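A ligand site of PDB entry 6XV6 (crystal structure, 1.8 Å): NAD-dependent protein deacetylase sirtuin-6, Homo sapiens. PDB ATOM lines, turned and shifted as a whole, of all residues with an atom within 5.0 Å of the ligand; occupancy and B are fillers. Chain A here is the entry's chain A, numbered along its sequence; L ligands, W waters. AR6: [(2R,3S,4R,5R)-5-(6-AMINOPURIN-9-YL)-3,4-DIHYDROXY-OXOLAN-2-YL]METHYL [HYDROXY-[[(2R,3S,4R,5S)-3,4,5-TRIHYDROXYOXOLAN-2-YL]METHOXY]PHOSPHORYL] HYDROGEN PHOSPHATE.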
ATOM      1  N   TYR A   3     -30.048   9.081  30.026  1.00  0.00           N
ATOM      2  CA  TYR A   3     -28.695   9.157  30.631  1.00  0.00           C
ATOM      3  C   TYR A   3     -27.699   9.689  29.597  1.00  0.00           C
ATOM      4  O   TYR A   3     -26.930  10.621  29.887  1.00  0.00           O
ATOM      5  CB  TYR A   3     -28.216   7.788  31.129  1.00  0.00           C
ATOM      6  CG  TYR A   3     -26.924   7.775  31.910  1.00  0.00           C
ATOM      7  CD1 TYR A   3     -26.574   8.768  32.818  1.00  0.00           C
ATOM      8  CD2 TYR A   3     -26.088   6.682  31.808  1.00  0.00           C
ATOM      9  CE1 TYR A   3     -25.417   8.672  33.572  1.00  0.00           C
ATOM     10  CE2 TYR A   3     -24.915   6.575  32.552  1.00  0.00           C
ATOM     11  CZ  TYR A   3     -24.577   7.564  33.455  1.00  0.00           C
ATOM     12  OH  TYR A   3     -23.419   7.402  34.173  1.00  0.00           O
ATOM     13  N   LEU A   7     -25.469  13.297  29.720  1.00  0.00           N
ATOM     14  CA  LEU A   7     -23.994  13.431  29.773  1.00  0.00           C
ATOM     15  C   LEU A   7     -23.446  13.874  28.408  1.00  0.00           C
ATOM     16  O   LEU A   7     -22.285  14.255  28.386  1.00  0.00           O
ATOM     17  CB  LEU A   7     -23.307  12.101  30.106  1.00  0.00           C
ATOM     18  CG  LEU A   7     -23.788  11.301  31.323  1.00  0.00           C
ATOM     19  CD1 LEU A   7     -23.234   9.898  31.278  1.00  0.00           C
ATOM     20  CD2 LEU A   7     -23.373  11.977  32.622  1.00  0.00           C
ATOM     21  N   GLU A  20     -12.573  -4.952  18.686  1.00  0.00           N
ATOM     22  CA  GLU A  20     -12.676  -6.103  19.630  1.00  0.00           C
ATOM     23  C   GLU A  20     -11.566  -7.106  19.330  1.00  0.00           C
ATOM     24  O   GLU A  20     -11.215  -7.258  18.192  1.00  0.00           O
ATOM     25  CB  GLU A  20     -14.033  -6.775  19.521  1.00  0.00           C
ATOM     26  CG  GLU A  20     -15.148  -5.870  19.908  1.00  0.00           C
ATOM     27  CD  GLU A  20     -16.529  -6.515  19.810  1.00  0.00           C
ATOM     28  OE1 GLU A  20     -16.729  -7.428  18.954  1.00  0.00           O
ATOM     29  OE2 GLU A  20     -17.387  -6.058  20.590  1.00  0.00           O
ATOM     30  N   GLY A  50     -18.529  -2.798  34.524  1.00  0.00           N
ATOM     31  CA  GLY A  50     -19.034  -1.717  33.678  1.00  0.00           C
ATOM     32  C   GLY A  50     -20.038  -2.244  32.690  1.00  0.00           C
ATOM     33  O   GLY A  50     -20.539  -3.415  32.855  1.00  0.00           O
ATOM     34  N   ALA A  51     -20.341  -1.447  31.673  1.00  0.00           N
ATOM     35  CA  ALA A  51     -21.548  -1.632  30.842  1.00  0.00           C
ATOM     36  C   ALA A  51     -21.454  -2.919  30.036  1.00  0.00           C
ATOM     37  O   ALA A  51     -22.507  -3.433  29.587  1.00  0.00           O
ATOM     38  CB  ALA A  51     -21.739  -0.412  29.971  1.00  0.00           C
ATOM     39  N   GLY A  52     -20.263  -3.452  29.829  1.00  0.00           N
ATOM     40  CA  GLY A  52     -20.102  -4.658  29.019  1.00  0.00           C
ATOM     41  C   GLY A  52     -20.760  -5.891  29.664  1.00  0.00           C
ATOM     42  O   GLY A  52     -20.994  -6.879  28.944  1.00  0.00           O
ATOM     43  N   THR A  55     -24.566  -5.936  28.185  1.00  0.00           N
ATOM     44  CA  THR A  55     -24.830  -5.940  26.731  1.00  0.00           C
ATOM     45  C   THR A  55     -25.573  -7.227  26.351  1.00  0.00           C
ATOM     46  O   THR A  55     -26.458  -7.131  25.492  1.00  0.00           O
ATOM     47  CB  THR A  55     -23.543  -5.741  25.913  1.00  0.00           C
ATOM     48  OG1 THR A  55     -22.575  -6.751  26.240  1.00  0.00           O
ATOM     49  CG2 THR A  55     -22.984  -4.358  26.132  1.00  0.00           C
ATOM     50  N   ASP A  61     -23.493  -0.635  25.552  1.00  0.00           N
ATOM     51  CA  ASP A  61     -22.384   0.000  26.300  1.00  0.00           C
ATOM     52  C   ASP A  61     -22.152   1.407  25.743  1.00  0.00           C
ATOM     53  O   ASP A  61     -23.013   1.897  24.974  1.00  0.00           O
ATOM     54  CB  ASP A  61     -21.161  -0.906  26.304  1.00  0.00           C
ATOM     55  CG  ASP A  61     -20.522  -1.202  24.966  1.00  0.00           C
ATOM     56  OD1 ASP A  61     -20.725  -0.393  24.032  1.00  0.00           O
ATOM     57  OD2 ASP A  61     -19.823  -2.209  24.873  1.00  0.00           O
ATOM     58  N   PHE A  62     -21.074   2.072  26.159  1.00  0.00           N
ATOM     59  CA  PHE A  62     -20.783   3.473  25.765  1.00  0.00           C
ATOM     60  C   PHE A  62     -19.784   3.516  24.608  1.00  0.00           C
ATOM     61  O   PHE A  62     -19.980   4.339  23.702  1.00  0.00           O
ATOM     62  CB  PHE A  62     -20.326   4.275  26.977  1.00  0.00           C
ATOM     63  CG  PHE A  62     -21.414   4.461  28.005  1.00  0.00           C
ATOM     64  CD1 PHE A  62     -22.319   5.496  27.897  1.00  0.00           C
ATOM     65  CD2 PHE A  62     -21.561   3.537  29.028  1.00  0.00           C
ATOM     66  CE1 PHE A  62     -23.340   5.637  28.827  1.00  0.00           C
ATOM     67  CE2 PHE A  62     -22.596   3.674  29.940  1.00  0.00           C
ATOM     68  CZ  PHE A  62     -23.491   4.706  29.829  1.00  0.00           C
ATOM     69  N   ARG A  63     -18.759   2.656  24.610  1.00  0.00           N
ATOM     70  CA  ARG A  63     -17.575   2.823  23.716  1.00  0.00           C
ATOM     71  C   ARG A  63     -17.335   1.577  22.870  1.00  0.00           C
ATOM     72  O   ARG A  63     -16.361   1.594  22.077  1.00  0.00           O
ATOM     73  CB  ARG A  63     -16.341   3.147  24.542  1.00  0.00           C
ATOM     74  CG  ARG A  63     -16.376   4.531  25.151  1.00  0.00           C
ATOM     75  CD  ARG A  63     -15.374   4.674  26.284  1.00  0.00           C
ATOM     76  NE  ARG A  63     -15.741   5.914  26.886  1.00  0.00           N
ATOM     77  CZ  ARG A  63     -16.538   6.094  27.928  1.00  0.00           C
ATOM     78  NH1 ARG A  63     -16.992   5.077  28.660  1.00  0.00           N
ATOM     79  NH2 ARG A  63     -16.796   7.326  28.274  1.00  0.00           N
ATOM     80  N   GLY A  64     -18.167   0.549  22.986  1.00  0.00           N
ATOM     81  CA  GLY A  64     -18.051  -0.636  22.126  1.00  0.00           C
ATOM     82  C   GLY A  64     -18.378  -0.253  20.683  1.00  0.00           C
ATOM     83  O   GLY A  64     -18.793   0.888  20.410  1.00  0.00           O
ATOM     84  N   TRP A  69     -21.678   6.281  22.547  1.00  0.00           N
ATOM     85  CA  TRP A  69     -20.801   7.327  21.950  1.00  0.00           C
ATOM     86  C   TRP A  69     -20.355   6.959  20.538  1.00  0.00           C
ATOM     87  O   TRP A  69     -20.346   7.829  19.682  1.00  0.00           O
ATOM     88  CB  TRP A  69     -19.598   7.631  22.854  1.00  0.00           C
ATOM     89  CG  TRP A  69     -19.948   7.965  24.263  1.00  0.00           C
ATOM     90  CD1 TRP A  69     -19.271   7.595  25.380  1.00  0.00           C
ATOM     91  CD2 TRP A  69     -21.056   8.749  24.714  1.00  0.00           C
ATOM     92  NE1 TRP A  69     -19.889   8.088  26.492  1.00  0.00           N
ATOM     93  CE2 TRP A  69     -20.978   8.797  26.121  1.00  0.00           C
ATOM     94  CE3 TRP A  69     -22.095   9.417  24.083  1.00  0.00           C
ATOM     95  CZ2 TRP A  69     -21.916   9.478  26.894  1.00  0.00           C
ATOM     96  CZ3 TRP A  69     -23.028  10.083  24.840  1.00  0.00           C
ATOM     97  CH2 TRP A  69     -22.924  10.125  26.229  1.00  0.00           C
ATOM     98  N   GLN A 111     -19.797   0.728  37.858  1.00  0.00           N
ATOM     99  CA  GLN A 111     -20.062   2.020  37.194  1.00  0.00           C
ATOM    100  C   GLN A 111     -21.454   2.016  36.574  1.00  0.00           C
ATOM    101  O   GLN A 111     -21.854   3.073  36.069  1.00  0.00           O
ATOM    102  CB  GLN A 111     -18.960   2.220  36.149  1.00  0.00           C
ATOM    103  CG  GLN A 111     -17.598   2.375  36.774  1.00  0.00           C
ATOM    104  CD  GLN A 111     -16.531   2.358  35.728  1.00  0.00           C
ATOM    105  OE1 GLN A 111     -16.391   3.328  34.971  1.00  0.00           O
ATOM    106  NE2 GLN A 111     -15.822   1.240  35.641  1.00  0.00           N
ATOM    107  N   ASN A 112     -22.175   0.891  36.613  1.00  0.00           N
ATOM    108  CA  ASN A 112     -23.459   0.732  35.902  1.00  0.00           C
ATOM    109  C   ASN A 112     -24.596   1.417  36.659  1.00  0.00           C
ATOM    110  O   ASN A 112     -24.708   1.206  37.870  1.00  0.00           O
ATOM    111  CB  ASN A 112     -23.792  -0.740  35.658  1.00  0.00           C
ATOM    112  CG  ASN A 112     -22.817  -1.392  34.707  1.00  0.00           C
ATOM    113  OD1 ASN A 112     -22.057  -0.693  34.023  1.00  0.00           O
ATOM    114  ND2 ASN A 112     -22.814  -2.713  34.671  1.00  0.00           N
ATOM    115  N   HIS A 131     -21.724   5.514  40.029  1.00  0.00           N
ATOM    116  CA  HIS A 131     -22.343   6.500  39.118  1.00  0.00           C
ATOM    117  C   HIS A 131     -23.849   6.613  39.372  1.00  0.00           C
ATOM    118  O   HIS A 131     -24.480   7.421  38.663  1.00  0.00           O
ATOM    119  CB  HIS A 131     -21.997   6.193  37.651  1.00  0.00           C
ATOM    120  CG  HIS A 131     -20.537   6.168  37.384  1.00  0.00           C
ATOM    121  ND1 HIS A 131     -20.004   5.604  36.229  1.00  0.00           N
ATOM    122  CD2 HIS A 131     -19.495   6.663  38.093  1.00  0.00           C
ATOM    123  CE1 HIS A 131     -18.685   5.747  36.259  1.00  0.00           C
ATOM    124  NE2 HIS A 131     -18.351   6.362  37.400  1.00  0.00           N
ATOM    125  N   GLY A 212     -16.013  -6.073  31.640  1.00  0.00           N
ATOM    126  CA  GLY A 212     -16.810  -5.217  30.752  1.00  0.00           C
ATOM    127  C   GLY A 212     -16.707  -3.746  31.101  1.00  0.00           C
ATOM    128  O   GLY A 212     -17.727  -3.049  31.026  1.00  0.00           O
ATOM    129  N   THR A 213     -15.512  -3.265  31.453  1.00  0.00           N
ATOM    130  CA  THR A 213     -15.250  -1.813  31.551  1.00  0.00           C
ATOM    131  C   THR A 213     -13.958  -1.483  30.789  1.00  0.00           C
ATOM    132  O   THR A 213     -12.982  -2.264  30.893  1.00  0.00           O
ATOM    133  CB  THR A 213     -15.223  -1.343  33.003  1.00  0.00           C
ATOM    134  OG1 THR A 213     -14.849   0.033  33.003  1.00  0.00           O
ATOM    135  CG2 THR A 213     -14.299  -2.131  33.891  1.00  0.00           C
ATOM    136  N   SER A 214     -13.970  -0.366  30.059  1.00  0.00           N
ATOM    137  CA  SER A 214     -12.805   0.149  29.305  1.00  0.00           C
ATOM    138  C   SER A 214     -11.883   0.914  30.257  1.00  0.00           C
ATOM    139  O   SER A 214     -10.742   1.250  29.815  1.00  0.00           O
ATOM    140  CB  SER A 214     -13.241   0.988  28.132  1.00  0.00           C
ATOM    141  OG  SER A 214     -13.878   2.141  28.587  1.00  0.00           O
ATOM    142  N   LEU A 215     -12.317   1.174  31.509  1.00  0.00           N
ATOM    143  CA  LEU A 215     -11.538   1.828  32.602  1.00  0.00           C
ATOM    144  C   LEU A 215     -11.102   3.235  32.203  1.00  0.00           C
ATOM    145  O   LEU A 215     -10.112   3.751  32.764  1.00  0.00           O
ATOM    146  CB  LEU A 215     -10.324   0.956  32.929  1.00  0.00           C
ATOM    147  CG  LEU A 215     -10.634  -0.443  33.450  1.00  0.00           C
ATOM    148  CD1 LEU A 215      -9.398  -1.306  33.537  1.00  0.00           C
ATOM    149  CD2 LEU A 215     -11.380  -0.364  34.785  1.00  0.00           C
ATOM    150  N   ILE A 217     -12.920   6.085  32.626  1.00  0.00           N
ATOM    151  CA  ILE A 217     -13.579   7.159  33.408  1.00  0.00           C
ATOM    152  C   ILE A 217     -13.006   7.138  34.830  1.00  0.00           C
ATOM    153  O   ILE A 217     -13.048   6.079  35.476  1.00  0.00           O
ATOM    154  CB  ILE A 217     -15.116   7.016  33.373  1.00  0.00           C
ATOM    155  CG1 ILE A 217     -15.666   7.192  31.961  1.00  0.00           C
ATOM    156  CG2 ILE A 217     -15.773   7.995  34.340  1.00  0.00           C
ATOM    157  CD1 ILE A 217     -15.432   8.560  31.339  1.00  0.00           C
ATOM    158  N   VAL A 237     -10.967  -8.416  32.101  1.00  0.00           N
ATOM    159  CA  VAL A 237     -11.790  -9.187  31.131  1.00  0.00           C
ATOM    160  C   VAL A 237     -12.541  -8.158  30.299  1.00  0.00           C
ATOM    161  O   VAL A 237     -13.355  -7.363  30.878  1.00  0.00           O
ATOM    162  CB  VAL A 237     -12.757 -10.147  31.822  1.00  0.00           C
ATOM    163  CG1 VAL A 237     -13.516 -10.983  30.820  1.00  0.00           C
ATOM    164  CG2 VAL A 237     -12.034 -11.050  32.817  1.00  0.00           C
ATOM    165  N   ASN A 238     -12.287  -8.138  28.992  1.00  0.00           N
ATOM    166  CA  ASN A 238     -12.839  -7.062  28.126  1.00  0.00           C
ATOM    167  C   ASN A 238     -12.594  -7.414  26.670  1.00  0.00           C
ATOM    168  O   ASN A 238     -11.502  -7.958  26.380  1.00  0.00           O
ATOM    169  CB  ASN A 238     -12.249  -5.696  28.483  1.00  0.00           C
ATOM    170  CG  ASN A 238     -13.229  -4.589  28.151  1.00  0.00           C
ATOM    171  OD1 ASN A 238     -14.299  -4.558  28.753  1.00  0.00           O
ATOM    172  ND2 ASN A 238     -12.879  -3.673  27.236  1.00  0.00           N
ATOM    173  N   LEU A 239     -13.559  -7.144  25.797  1.00  0.00           N
ATOM    174  CA  LEU A 239     -13.387  -7.401  24.346  1.00  0.00           C
ATOM    175  C   LEU A 239     -12.459  -6.344  23.733  1.00  0.00           C
ATOM    176  O   LEU A 239     -11.625  -6.712  22.885  1.00  0.00           O
ATOM    177  CB  LEU A 239     -14.738  -7.424  23.626  1.00  0.00           C
ATOM    178  CG  LEU A 239     -15.585  -8.653  23.895  1.00  0.00           C
ATOM    179  CD1 LEU A 239     -17.007  -8.476  23.366  1.00  0.00           C
ATOM    180  CD2 LEU A 239     -14.944  -9.876  23.303  1.00  0.00           C
ATOM    181  N   GLN A 240     -12.590  -5.093  24.129  1.00  0.00           N
ATOM    182  CA  GLN A 240     -11.698  -4.010  23.637  1.00  0.00           C
ATOM    183  C   GLN A 240     -10.476  -3.898  24.523  1.00  0.00           C
ATOM    184  O   GLN A 240     -10.484  -4.324  25.695  1.00  0.00           O
ATOM    185  CB  GLN A 240     -12.426  -2.670  23.591  1.00  0.00           C
ATOM    186  CG  GLN A 240     -13.460  -2.545  22.493  1.00  0.00           C
ATOM    187  CD  GLN A 240     -14.179  -1.231  22.589  1.00  0.00           C
ATOM    188  OE1 GLN A 240     -14.395  -0.681  23.681  1.00  0.00           O
ATOM    189  NE2 GLN A 240     -14.580  -0.700  21.438  1.00  0.00           N
ATOM    190  N   PRO A 241      -9.393  -3.279  24.006  1.00  0.00           N
ATOM    191  CA  PRO A 241      -8.315  -2.779  24.859  1.00  0.00           C
ATOM    192  C   PRO A 241      -8.915  -1.872  25.939  1.00  0.00           C
ATOM    193  O   PRO A 241      -9.992  -1.348  25.738  1.00  0.00           O
ATOM    194  CB  PRO A 241      -7.452  -1.915  23.920  1.00  0.00           C
ATOM    195  CG  PRO A 241      -7.736  -2.483  22.534  1.00  0.00           C
ATOM    196  CD  PRO A 241      -9.178  -2.945  22.583  1.00  0.00           C
ATOM    197  N   GLY A 254     -12.681 -11.969  25.630  1.00  0.00           N
ATOM    198  CA  GLY A 254     -13.789 -12.864  25.313  1.00  0.00           C
ATOM    199  C   GLY A 254     -15.076 -12.286  25.866  1.00  0.00           C
ATOM    200  O   GLY A 254     -14.986 -11.319  26.618  1.00  0.00           O
ATOM    201  N   TYR A 255     -16.210 -12.881  25.517  1.00  0.00           N
ATOM    202  CA  TYR A 255     -17.508 -12.524  26.094  1.00  0.00           C
ATOM    203  C   TYR A 255     -17.483 -12.853  27.582  1.00  0.00           C
ATOM    204  O   TYR A 255     -17.136 -13.998  27.945  1.00  0.00           O
ATOM    205  CB  TYR A 255     -18.623 -13.237  25.340  1.00  0.00           C
ATOM    206  CG  TYR A 255     -18.716 -12.828  23.899  1.00  0.00           C
ATOM    207  CD1 TYR A 255     -19.296 -11.614  23.540  1.00  0.00           C
ATOM    208  CD2 TYR A 255     -18.250 -13.648  22.899  1.00  0.00           C
ATOM    209  CE1 TYR A 255     -19.373 -11.226  22.219  1.00  0.00           C
ATOM    210  CE2 TYR A 255     -18.391 -13.305  21.560  1.00  0.00           C
ATOM    211  CZ  TYR A 255     -18.988 -12.094  21.226  1.00  0.00           C
ATOM    212  OH  TYR A 255     -19.066 -11.720  19.919  1.00  0.00           O
ATOM    213  N   VAL A 256     -17.824 -11.884  28.409  1.00  0.00           N
ATOM    214  CA  VAL A 256     -17.776 -12.037  29.886  1.00  0.00           C
ATOM    215  C   VAL A 256     -18.677 -13.207  30.308  1.00  0.00           C
ATOM    216  O   VAL A 256     -18.254 -13.960  31.189  1.00  0.00           O
ATOM    217  CB  VAL A 256     -18.106 -10.707  30.589  1.00  0.00           C
ATOM    218  CG1 VAL A 256     -19.518 -10.176  30.303  1.00  0.00           C
ATOM    219  CG2 VAL A 256     -17.849 -10.851  32.066  1.00  0.00           C
HETATM  220  N1  AR6 L   1     -17.967  -9.239  27.092  1.00  0.00           N
HETATM  221  C2  AR6 L   1     -16.828  -8.577  27.325  1.00  0.00           C
HETATM  222  N3  AR6 L   1     -16.531  -7.288  27.101  1.00  0.00           N
HETATM  223  C4  AR6 L   1     -17.609  -6.636  26.621  1.00  0.00           C
HETATM  224  C5  AR6 L   1     -18.854  -7.184  26.356  1.00  0.00           C
HETATM  225  C6  AR6 L   1     -19.033  -8.561  26.595  1.00  0.00           C
HETATM  226  N6  AR6 L   1     -20.200  -9.208  26.417  1.00  0.00           N
HETATM  227  N7  AR6 L   1     -19.711  -6.201  25.866  1.00  0.00           N
HETATM  228  C8  AR6 L   1     -18.989  -5.110  25.877  1.00  0.00           C
HETATM  229  N9  AR6 L   1     -17.694  -5.310  26.298  1.00  0.00           N
HETATM  230  PA  AR6 L   1     -17.539   1.339  28.188  1.00  0.00           P
HETATM  231  PB  AR6 L   1     -17.895   1.638  31.034  1.00  0.00           P
HETATM  232  C1' AR6 L   1     -16.680  -4.291  26.524  1.00  0.00           C
HETATM  233  O1A AR6 L   1     -16.494   2.405  28.294  1.00  0.00           O
HETATM  234  O1B AR6 L   1     -18.892   0.981  31.974  1.00  0.00           O
HETATM  235  C1D AR6 L   1     -19.975   6.639  31.050  1.00  0.00           C
HETATM  236  O1D AR6 L   1     -19.774   8.057  31.073  1.00  0.00           O
HETATM  237  C2' AR6 L   1     -16.497  -3.263  25.409  1.00  0.00           C
HETATM  238  O2' AR6 L   1     -15.516  -3.740  24.528  1.00  0.00           O
HETATM  239  O2A AR6 L   1     -18.496   1.253  27.069  1.00  0.00           O
HETATM  240  O2B AR6 L   1     -16.453   1.284  31.171  1.00  0.00           O
HETATM  241  C2D AR6 L   1     -20.840   6.130  32.219  1.00  0.00           C
HETATM  242  O2D AR6 L   1     -20.830   6.968  33.373  1.00  0.00           O
HETATM  243  C3' AR6 L   1     -16.065  -1.995  26.167  1.00  0.00           C
HETATM  244  O3' AR6 L   1     -14.669  -1.748  26.104  1.00  0.00           O
HETATM  245  O3A AR6 L   1     -18.379   1.337  29.553  1.00  0.00           O
HETATM  246  C3D AR6 L   1     -20.212   4.775  32.541  1.00  0.00           C
HETATM  247  O3D AR6 L   1     -20.482   4.268  33.850  1.00  0.00           O
HETATM  248  C4' AR6 L   1     -16.430  -2.270  27.615  1.00  0.00           C
HETATM  249  O4' AR6 L   1     -17.112  -3.533  27.618  1.00  0.00           O
HETATM  250  C4D AR6 L   1     -18.733   5.154  32.385  1.00  0.00           C
HETATM  251  O4D AR6 L   1     -18.712   6.004  31.204  1.00  0.00           O
HETATM  252  C5' AR6 L   1     -17.348  -1.272  28.248  1.00  0.00           C
HETATM  253  O5' AR6 L   1     -16.687  -0.002  28.291  1.00  0.00           O
HETATM  254  C5D AR6 L   1     -17.762   4.011  32.224  1.00  0.00           C
HETATM  255  O5D AR6 L   1     -18.102   3.238  31.055  1.00  0.00           O
HETATM  256  O   HOH W   1     -23.793   3.587  33.714  1.00  0.00           O
HETATM  257  O   HOH W   2     -19.627  -3.842  22.794  1.00  0.00           O
HETATM  258  O   HOH W   3     -22.774  -9.022  28.492  1.00  0.00           O
HETATM  259  O   HOH W   4     -17.119  -4.609  22.517  1.00  0.00           O
HETATM  260  O   HOH W   5     -21.308 -11.503  27.750  1.00  0.00           O
HETATM  261  O   HOH W   6     -21.221   1.794  32.924  1.00  0.00           O
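N of Gln 240 sits close to O2' of the ligand (3.2 Å).
N of Phe 62 sits at hydrogen-bond distance from O2A of the ligand, 2.9 Å away.
An oxygen (O3D) of the ligand is in hydrogen-bond range of a ring nitrogen (ND1) of His 131 (2.8 Å).
The backbone NH of Val 256 sits at hydrogen-bond distance from a nitrogen (N1) of the ligand.
The backbone NH (N) of Ala 51 is in hydrogen-bond range of an oxygen (O1B) of the ligand.
The guanidinium group (NH1) of Arg 63 lies within salt-bridge range of an oxygen (O1A) of the ligand (2.7 Å).
An oxygen (O3') of the ligand lies within hydrogen-bond range of the side-chain amide nitrogen of Asn 238 (2.9 Å).
The side-chain hydroxyl of Ser 214 sits at hydrogen-bond distance from an oxygen (O1A) of the ligand (2.6 Å).
The backbone NH of Arg 63 lies within hydrogen-bond range of an oxygen (O2A) of the ligand (2.8 Å).
A nitrogen (N3) of the ligand sits at hydrogen-bond distance from the backbone NH (N) of Leu 239, 3.2 Å away.
N of Ser 214 is in hydrogen-bond range of O2B of the ligand (3.2 Å).
OH of Tyr 3 lies within hydrogen-bond range of O2D of the ligand.
OG1 of Thr 213 lies within hydrogen-bond range of O2B of the ligand, 2.7 Å away.
OE1 of Gln 240 is in hydrogen-bond range of O3' of the ligand (2.7 Å).
O3D of the ligand is in hydrogen-bond range of O of Gln 111, at 2.9 Å.
The side-chain hydroxyl (OG1) of Thr 55 is in hydrogen-bond range of a nitrogen (N7) of the ligand, at 2.9 Å.
The backbone NH of Gly 212 sits at hydrogen-bond distance from the backbone carbonyl oxygen of Val 237, at 3.1 Å.
N of Leu 215 is in hydrogen-bond range of OG1 of Thr 213, 3.2 Å away.
The backbone carbonyl oxygen of Phe 62 is in hydrogen-bond range of the backbone NH of Trp 69 (2.8 Å).
The backbone NH (N) of Thr 213 lies within hydrogen-bond range of the side-chain amide oxygen (OD1) of Asn 238, at 3.2 Å.
The backbone carbonyl oxygen (O) of Gln 111 lies within hydrogen-bond range of a ring nitrogen (ND1) of His 131 (3.1 Å).
The backbone NH (N) of Gly 64 lies within hydrogen-bond range of the side-chain carboxylate (OD1) of Asp 61, at 2.9 Å.
O of Gln 240 lies within hydrogen-bond range of ND2 of Asn 238 (2.9 Å).
The backbone NH (N) of Ala 51 lies within hydrogen-bond range of the backbone carbonyl oxygen (O) of Gly 212 (3.1 Å).
A nitrogen (N7) of the ligand sits close to the backbone carbonyl oxygen (O) of Gly 52.
The backbone carbonyl oxygen of Gly 212 sits close to an oxygen (O4') of the ligand, at 3.5 Å.
Residues that only touch the ligand: Asp 61 (3.2 Å), Gly 50 (3.2 Å), Ile 217 (3.4 Å), Gly 254 (3.4 Å), Tyr 255 (3.5 Å) and Leu 7 (3.9 Å).
21 residues have an atom within 4 Å of the ligand: Tyr 3, Leu 7, Gly 50, Ala 51, Gly 52, Thr 55, Asp 61, Phe 62, Arg 63, Gln 111, His 131, Gly 212, Thr 213, Ser 214, Ile 217, Asn 238, Leu 239, Gln 240, Gly 254, Tyr 255 and Val 256.
Water W6 lies within hydrogen-bond range of an oxygen (O1B) of the ligand (2.6 Å), the side-chain amide oxygen of Asn 112 (2.8 Å) and the backbone carbonyl oxygen of Gln 111 (3.5 Å).
Water W4 lies within hydrogen-bond range of the side-chain carboxylate (OE2) of Glu 20 and an oxygen (O2') of the ligand.
Water W3 lies within hydrogen-bond range of the backbone carbonyl oxygen of Gly 52 (2.8 Å), the side-chain hydroxyl of Thr 55 (3.2 Å) and a nitrogen (N6) of the ligand (3.3 Å).
Water W1 lies within hydrogen-bond range of the backbone carbonyl oxygen of Gln 111 and an oxygen (O3D) of the ligand.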
